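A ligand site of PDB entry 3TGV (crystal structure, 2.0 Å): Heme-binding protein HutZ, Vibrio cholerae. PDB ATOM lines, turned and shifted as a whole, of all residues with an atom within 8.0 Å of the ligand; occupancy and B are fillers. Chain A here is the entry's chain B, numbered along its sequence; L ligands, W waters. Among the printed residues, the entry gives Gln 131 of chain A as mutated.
The guanidinium group (NH2) of Arg 11 lies within salt-bridge range of an oxygen (O2) of the ligand (2.4 Å). The side-chain amide oxygen (OE1) of Gln 37 sits close to an oxygen (O2) of the ligand (3.3 Å). The side-chain hydroxyl (OH) of Tyr 42 lies within hydrogen-bond range of an oxygen (O2) of the ligand, 3.0 Å away.
N of Ile 64 is in hydrogen-bond range of O of Phe 84, 2.8 Å away. The guanidinium group of Arg 11 sits at hydrogen-bond distance from the side-chain hydroxyl of Tyr 42 (2.9 Å). O of Tyr 42 lies within hydrogen-bond range of N of Leu 127, 2.7 Å away. The guanidinium group of Arg 11 lies within hydrogen-bond range of the side-chain amide oxygen of Gln 37 (3.2 Å).
Merely in contact with the ligand: Phe 84 (3.7 Å), Pro 129 (3.2 Å) and Leu 133 (3.7 Å). Hydrophobic or aromatic side chains that line the ligand: Tyr 42, Phe 84, Pro 129 and Leu 133. The nearest printed residue that does not touch the ligand is Gly 132 (4.001 Å).
Water W1 bridges O1 of the ligand (3.1 Å) and OE1 of Gln 37 (3.4 Å).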
ATOM      1  N   ILE A   7     -14.636   0.898 -25.488  1.00  0.00           N
ATOM      2  CA  ILE A   7     -14.145   1.000 -24.114  1.00  0.00           C
ATOM      3  C   ILE A   7     -12.786   0.307 -23.980  1.00  0.00           C
ATOM      4  O   ILE A   7     -11.861   0.850 -23.367  1.00  0.00           O
ATOM      5  CB  ILE A   7     -15.125   0.370 -23.103  1.00  0.00           C
ATOM      6  CG1 ILE A   7     -16.435   1.164 -23.074  1.00  0.00           C
ATOM      7  CG2 ILE A   7     -14.535   0.343 -21.733  1.00  0.00           C
ATOM      8  CD1 ILE A   7     -17.537   0.482 -22.274  1.00  0.00           C
ATOM      9  N   ARG A  11      -9.261   2.176 -22.617  1.00  0.00           N
ATOM     10  CA  ARG A  11      -8.492   1.802 -21.419  1.00  0.00           C
ATOM     11  C   ARG A  11      -7.058   1.383 -21.751  1.00  0.00           C
ATOM     12  O   ARG A  11      -6.168   1.447 -20.892  1.00  0.00           O
ATOM     13  CB  ARG A  11      -9.171   0.662 -20.656  1.00  0.00           C
ATOM     14  CG  ARG A  11     -10.604   0.926 -20.274  1.00  0.00           C
ATOM     15  CD  ARG A  11     -11.299  -0.399 -19.907  1.00  0.00           C
ATOM     16  NE  ARG A  11     -11.098  -0.718 -18.513  1.00  0.00           N
ATOM     17  CZ  ARG A  11     -11.115  -1.937 -17.982  1.00  0.00           C
ATOM     18  NH1 ARG A  11     -11.341  -3.015 -18.719  1.00  0.00           N
ATOM     19  NH2 ARG A  11     -10.911  -2.068 -16.676  1.00  0.00           N
ATOM     20  N   GLN A  37      -3.818  -1.587 -14.763  1.00  0.00           N
ATOM     21  CA  GLN A  37      -5.000  -2.268 -14.243  1.00  0.00           C
ATOM     22  C   GLN A  37      -4.789  -3.758 -14.412  1.00  0.00           C
ATOM     23  O   GLN A  37      -4.179  -4.195 -15.381  1.00  0.00           O
ATOM     24  CB  GLN A  37      -6.263  -1.826 -14.990  1.00  0.00           C
ATOM     25  CG  GLN A  37      -7.566  -2.297 -14.337  1.00  0.00           C
ATOM     26  CD  GLN A  37      -8.161  -3.559 -14.964  1.00  0.00           C
ATOM     27  OE1 GLN A  37      -9.319  -3.931 -14.687  1.00  0.00           O
ATOM     28  NE2 GLN A  37      -7.391  -4.231 -15.807  1.00  0.00           N
ATOM     29  N   ASN A  38      -5.271  -4.523 -13.457  1.00  0.00           N
ATOM     30  CA  ASN A  38      -5.309  -5.966 -13.600  1.00  0.00           C
ATOM     31  C   ASN A  38      -6.461  -6.494 -12.738  1.00  0.00           C
ATOM     32  O   ASN A  38      -7.248  -5.699 -12.228  1.00  0.00           O
ATOM     33  CB  ASN A  38      -3.972  -6.569 -13.176  1.00  0.00           C
ATOM     34  CG  ASN A  38      -3.606  -6.215 -11.754  1.00  0.00           C
ATOM     35  OD1 ASN A  38      -4.341  -6.533 -10.837  1.00  0.00           O
ATOM     36  ND2 ASN A  38      -2.471  -5.545 -11.573  1.00  0.00           N
ATOM     37  N   GLN A  39      -6.542  -7.802 -12.563  1.00  0.00           N
ATOM     38  CA  GLN A  39      -7.673  -8.395 -11.845  1.00  0.00           C
ATOM     39  C   GLN A  39      -7.727  -8.037 -10.367  1.00  0.00           C
ATOM     40  O   GLN A  39      -8.712  -8.342  -9.688  1.00  0.00           O
ATOM     41  CB  GLN A  39      -7.691  -9.914 -12.020  1.00  0.00           C
ATOM     42  CG  GLN A  39      -6.507 -10.618 -11.386  1.00  0.00           C
ATOM     43  CD  GLN A  39      -6.728 -12.119 -11.262  1.00  0.00           C
ATOM     44  OE1 GLN A  39      -7.444 -12.725 -12.065  1.00  0.00           O
ATOM     45  NE2 GLN A  39      -6.121 -12.723 -10.247  1.00  0.00           N
ATOM     46  N   GLY A  41      -7.270  -4.798  -9.382  1.00  0.00           N
ATOM     47  CA  GLY A  41      -7.729  -3.431  -9.318  1.00  0.00           C
ATOM     48  C   GLY A  41      -6.872  -2.499 -10.160  1.00  0.00           C
ATOM     49  O   GLY A  41      -6.128  -2.952 -11.031  1.00  0.00           O
ATOM     50  N   TYR A  42      -6.995  -1.204  -9.910  1.00  0.00           N
ATOM     51  CA  TYR A  42      -6.185  -0.187 -10.547  1.00  0.00           C
ATOM     52  C   TYR A  42      -5.031   0.167  -9.628  1.00  0.00           C
ATOM     53  O   TYR A  42      -5.192   0.213  -8.406  1.00  0.00           O
ATOM     54  CB  TYR A  42      -7.021   1.062 -10.822  1.00  0.00           C
ATOM     55  CG  TYR A  42      -7.965   0.891 -11.987  1.00  0.00           C
ATOM     56  CD1 TYR A  42      -7.644   1.399 -13.238  1.00  0.00           C
ATOM     57  CD2 TYR A  42      -9.158   0.197 -11.848  1.00  0.00           C
ATOM     58  CE1 TYR A  42      -8.509   1.232 -14.319  1.00  0.00           C
ATOM     59  CE2 TYR A  42     -10.015   0.024 -12.915  1.00  0.00           C
ATOM     60  CZ  TYR A  42      -9.693   0.547 -14.147  1.00  0.00           C
ATOM     61  OH  TYR A  42     -10.535   0.373 -15.229  1.00  0.00           O
ATOM     62  N   ILE A  64     -12.125   8.690  -9.490  1.00  0.00           N
ATOM     63  CA  ILE A  64     -11.155   8.440 -10.540  1.00  0.00           C
ATOM     64  C   ILE A  64     -11.756   8.751 -11.901  1.00  0.00           C
ATOM     65  O   ILE A  64     -12.920   8.431 -12.167  1.00  0.00           O
ATOM     66  CB  ILE A  64     -10.732   6.981 -10.526  1.00  0.00           C
ATOM     67  CG1 ILE A  64     -10.035   6.670  -9.193  1.00  0.00           C
ATOM     68  CG2 ILE A  64      -9.854   6.665 -11.740  1.00  0.00           C
ATOM     69  CD1 ILE A  64      -9.853   5.197  -8.899  1.00  0.00           C
ATOM     70  N   MET A  66     -10.770   8.599 -16.188  1.00  0.00           N
ATOM     71  CA  MET A  66      -9.928   8.394 -17.349  1.00  0.00           C
ATOM     72  C   MET A  66     -10.538   9.201 -18.510  1.00  0.00           C
ATOM     73  O   MET A  66     -11.679   8.959 -18.902  1.00  0.00           O
ATOM     74  CB  MET A  66      -9.908   6.898 -17.622  1.00  0.00           C
ATOM     75  CG  MET A  66      -8.788   6.405 -18.452  1.00  0.00           C
ATOM     76  SD  MET A  66      -9.086   4.665 -18.856  1.00  0.00           S
ATOM     77  CE  MET A  66      -9.155   3.959 -17.234  1.00  0.00           C
ATOM     78  N   LEU A  82     -14.286   7.941 -18.701  1.00  0.00           N
ATOM     79  CA  LEU A  82     -14.807   6.942 -17.773  1.00  0.00           C
ATOM     80  C   LEU A  82     -14.609   7.453 -16.358  1.00  0.00           C
ATOM     81  O   LEU A  82     -13.506   7.898 -16.007  1.00  0.00           O
ATOM     82  CB  LEU A  82     -14.059   5.614 -17.919  1.00  0.00           C
ATOM     83  CG  LEU A  82     -13.947   4.979 -19.292  1.00  0.00           C
ATOM     84  CD1 LEU A  82     -13.111   3.708 -19.229  1.00  0.00           C
ATOM     85  CD2 LEU A  82     -15.344   4.673 -19.845  1.00  0.00           C
ATOM     86  N   THR A  83     -15.643   7.397 -15.526  1.00  0.00           N
ATOM     87  CA  THR A  83     -15.469   7.841 -14.151  1.00  0.00           C
ATOM     88  C   THR A  83     -15.997   6.826 -13.158  1.00  0.00           C
ATOM     89  O   THR A  83     -17.049   6.215 -13.372  1.00  0.00           O
ATOM     90  CB  THR A  83     -16.151   9.196 -13.898  1.00  0.00           C
ATOM     91  OG1 THR A  83     -15.742  10.121 -14.920  1.00  0.00           O
ATOM     92  CG2 THR A  83     -15.739   9.752 -12.539  1.00  0.00           C
ATOM     93  N   PHE A  84     -15.280   6.659 -12.061  1.00  0.00           N
ATOM     94  CA  PHE A  84     -15.738   5.779 -10.990  1.00  0.00           C
ATOM     95  C   PHE A  84     -15.149   6.164  -9.641  1.00  0.00           C
ATOM     96  O   PHE A  84     -14.017   6.650  -9.569  1.00  0.00           O
ATOM     97  CB  PHE A  84     -15.441   4.311 -11.304  1.00  0.00           C
ATOM     98  CG  PHE A  84     -13.986   4.008 -11.562  1.00  0.00           C
ATOM     99  CD1 PHE A  84     -13.396   4.376 -12.761  1.00  0.00           C
ATOM    100  CD2 PHE A  84     -13.224   3.327 -10.626  1.00  0.00           C
ATOM    101  CE1 PHE A  84     -12.045   4.080 -13.006  1.00  0.00           C
ATOM    102  CE2 PHE A  84     -11.900   3.006 -10.866  1.00  0.00           C
ATOM    103  CZ  PHE A  84     -11.316   3.386 -12.059  1.00  0.00           C
ATOM    104  N   ASP A  85     -15.925   5.947  -8.584  1.00  0.00           N
ATOM    105  CA  ASP A  85     -15.419   6.091  -7.223  1.00  0.00           C
ATOM    106  C   ASP A  85     -14.730   4.802  -6.834  1.00  0.00           C
ATOM    107  O   ASP A  85     -15.052   3.738  -7.360  1.00  0.00           O
ATOM    108  CB  ASP A  85     -16.551   6.389  -6.243  1.00  0.00           C
ATOM    109  CG  ASP A  85     -17.306   7.658  -6.578  1.00  0.00           C
ATOM    110  OD1 ASP A  85     -16.666   8.689  -6.912  1.00  0.00           O
ATOM    111  OD2 ASP A  85     -18.556   7.624  -6.516  1.00  0.00           O
ATOM    112  N   ALA A  86     -13.783   4.884  -5.901  1.00  0.00           N
ATOM    113  CA  ALA A  86     -13.045   3.698  -5.512  1.00  0.00           C
ATOM    114  C   ALA A  86     -12.555   3.806  -4.074  1.00  0.00           C
ATOM    115  O   ALA A  86     -12.516   4.886  -3.496  1.00  0.00           O
ATOM    116  CB  ALA A  86     -11.864   3.468  -6.463  1.00  0.00           C
ATOM    117  N   LEU A 127      -6.481   0.647  -6.056  1.00  0.00           N
ATOM    118  CA  LEU A 127      -7.745   1.349  -6.091  1.00  0.00           C
ATOM    119  C   LEU A 127      -8.822   0.403  -6.623  1.00  0.00           C
ATOM    120  O   LEU A 127      -8.719  -0.107  -7.739  1.00  0.00           O
ATOM    121  CB  LEU A 127      -7.613   2.577  -7.003  1.00  0.00           C
ATOM    122  CG  LEU A 127      -6.298   3.356  -6.925  1.00  0.00           C
ATOM    123  CD1 LEU A 127      -6.241   4.439  -7.991  1.00  0.00           C
ATOM    124  CD2 LEU A 127      -6.091   3.947  -5.532  1.00  0.00           C
ATOM    125  N   GLN A 128      -9.853   0.162  -5.821  1.00  0.00           N
ATOM    126  CA  GLN A 128     -10.879  -0.826  -6.184  1.00  0.00           C
ATOM    127  C   GLN A 128     -12.249  -0.179  -6.282  1.00  0.00           C
ATOM    128  O   GLN A 128     -12.700   0.469  -5.335  1.00  0.00           O
ATOM    129  CB  GLN A 128     -10.903  -1.953  -5.152  1.00  0.00           C
ATOM    130  CG  GLN A 128      -9.537  -2.208  -4.563  1.00  0.00           C
ATOM    131  CD  GLN A 128      -9.415  -3.566  -3.889  1.00  0.00           C
ATOM    132  OE1 GLN A 128      -8.929  -3.672  -2.762  1.00  0.00           O
ATOM    133  NE2 GLN A 128      -9.845  -4.609  -4.591  1.00  0.00           N
ATOM    134  N   PRO A 129     -12.934  -0.382  -7.419  1.00  0.00           N
ATOM    135  CA  PRO A 129     -14.249   0.224  -7.683  1.00  0.00           C
ATOM    136  C   PRO A 129     -15.346  -0.381  -6.830  1.00  0.00           C
ATOM    137  O   PRO A 129     -15.413  -1.604  -6.698  1.00  0.00           O
ATOM    138  CB  PRO A 129     -14.495  -0.103  -9.162  1.00  0.00           C
ATOM    139  CG  PRO A 129     -13.674  -1.337  -9.405  1.00  0.00           C
ATOM    140  CD  PRO A 129     -12.446  -1.150  -8.580  1.00  0.00           C
ATOM    141  N   GLU A 130     -16.204   0.473  -6.282  1.00  0.00           N
ATOM    142  CA  GLU A 130     -17.180   0.075  -5.268  1.00  0.00           C
ATOM    143  C   GLU A 130     -18.628   0.453  -5.639  1.00  0.00           C
ATOM    144  O   GLU A 130     -19.602  -0.063  -5.059  1.00  0.00           O
ATOM    145  CB  GLU A 130     -16.798   0.770  -3.957  1.00  0.00           C
ATOM    146  CG  GLU A 130     -17.351   0.116  -2.713  1.00  0.00           C
ATOM    147  CD  GLU A 130     -16.328  -0.791  -2.027  1.00  0.00           C
ATOM    148  OE1 GLU A 130     -16.193  -0.690  -0.789  1.00  0.00           O
ATOM    149  OE2 GLU A 130     -15.671  -1.592  -2.727  1.00  0.00           O
ATOM    150  N   GLN A 131     -18.781   1.361  -6.590  1.00  0.00           N
ATOM    151  CA  GLN A 131     -20.074   1.969  -6.858  1.00  0.00           C
ATOM    152  C   GLN A 131     -20.333   2.147  -8.357  1.00  0.00           C
ATOM    153  O   GLN A 131     -20.893   3.155  -8.787  1.00  0.00           O
ATOM    154  CB  GLN A 131     -20.210   3.301  -6.110  1.00  0.00           C
ATOM    155  CG  GLN A 131     -20.994   3.184  -4.814  1.00  0.00           C
ATOM    156  CD  GLN A 131     -20.119   3.313  -3.602  1.00  0.00           C
ATOM    157  OE1 GLN A 131     -19.247   4.190  -3.538  1.00  0.00           O
ATOM    158  NE2 GLN A 131     -20.321   2.435  -2.618  1.00  0.00           N
ATOM    159  N   GLY A 132     -19.915   1.166  -9.148  1.00  0.00           N
ATOM    160  CA  GLY A 132     -20.158   1.212 -10.563  1.00  0.00           C
ATOM    161  C   GLY A 132     -19.318   2.241 -11.299  1.00  0.00           C
ATOM    162  O   GLY A 132     -18.404   2.869 -10.750  1.00  0.00           O
ATOM    163  N   LEU A 133     -19.654   2.411 -12.565  1.00  0.00           N
ATOM    164  CA  LEU A 133     -18.803   3.101 -13.495  1.00  0.00           C
ATOM    165  C   LEU A 133     -19.683   3.962 -14.379  1.00  0.00           C
ATOM    166  O   LEU A 133     -20.738   3.516 -14.809  1.00  0.00           O
ATOM    167  CB  LEU A 133     -18.040   2.037 -14.313  1.00  0.00           C
ATOM    168  CG  LEU A 133     -17.229   2.385 -15.543  1.00  0.00           C
ATOM    169  CD1 LEU A 133     -18.074   3.192 -16.458  1.00  0.00           C
ATOM    170  CD2 LEU A 133     -15.961   3.175 -15.139  1.00  0.00           C
ATOM    171  N   PHE A 134     -19.261   5.193 -14.638  1.00  0.00           N
ATOM    172  CA  PHE A 134     -19.975   6.076 -15.548  1.00  0.00           C
ATOM    173  C   PHE A 134     -19.202   6.185 -16.869  1.00  0.00           C
ATOM    174  O   PHE A 134     -18.002   6.482 -16.889  1.00  0.00           O
ATOM    175  CB  PHE A 134     -20.179   7.450 -14.921  1.00  0.00           C
ATOM    176  CG  PHE A 134     -21.091   7.445 -13.716  1.00  0.00           C
ATOM    177  CD1 PHE A 134     -22.445   7.774 -13.847  1.00  0.00           C
ATOM    178  CD2 PHE A 134     -20.611   7.109 -12.462  1.00  0.00           C
ATOM    179  CE1 PHE A 134     -23.289   7.765 -12.745  1.00  0.00           C
ATOM    180  CE2 PHE A 134     -21.448   7.112 -11.359  1.00  0.00           C
ATOM    181  CZ  PHE A 134     -22.789   7.441 -11.496  1.00  0.00           C
HETATM  182  C1  LIG L   1     -13.400  -2.523 -14.372  1.00  0.00           C
HETATM  183  O1  LIG L   1     -13.624  -3.990 -14.234  1.00  0.00           O
HETATM  184  O2  LIG L   1     -12.117  -2.106 -14.599  1.00  0.00           O
HETATM  185  C2  LIG L   1     -14.249  -1.629 -13.589  1.00  0.00           C
HETATM  186  C3  LIG L   1     -13.830  -0.275 -13.350  1.00  0.00           C
HETATM  187  C4  LIG L   1     -14.632   0.548 -12.590  1.00  0.00           C
HETATM  188  C5  LIG L   1     -15.872   0.052 -12.039  1.00  0.00           C
HETATM  189  C6  LIG L   1     -16.266  -1.286 -12.271  1.00  0.00           C
HETATM  190  C7  LIG L   1     -15.442  -2.121 -13.053  1.00  0.00           C
HETATM  191  O   HOH W   1     -11.903  -5.642 -16.197  1.00  0.00           O
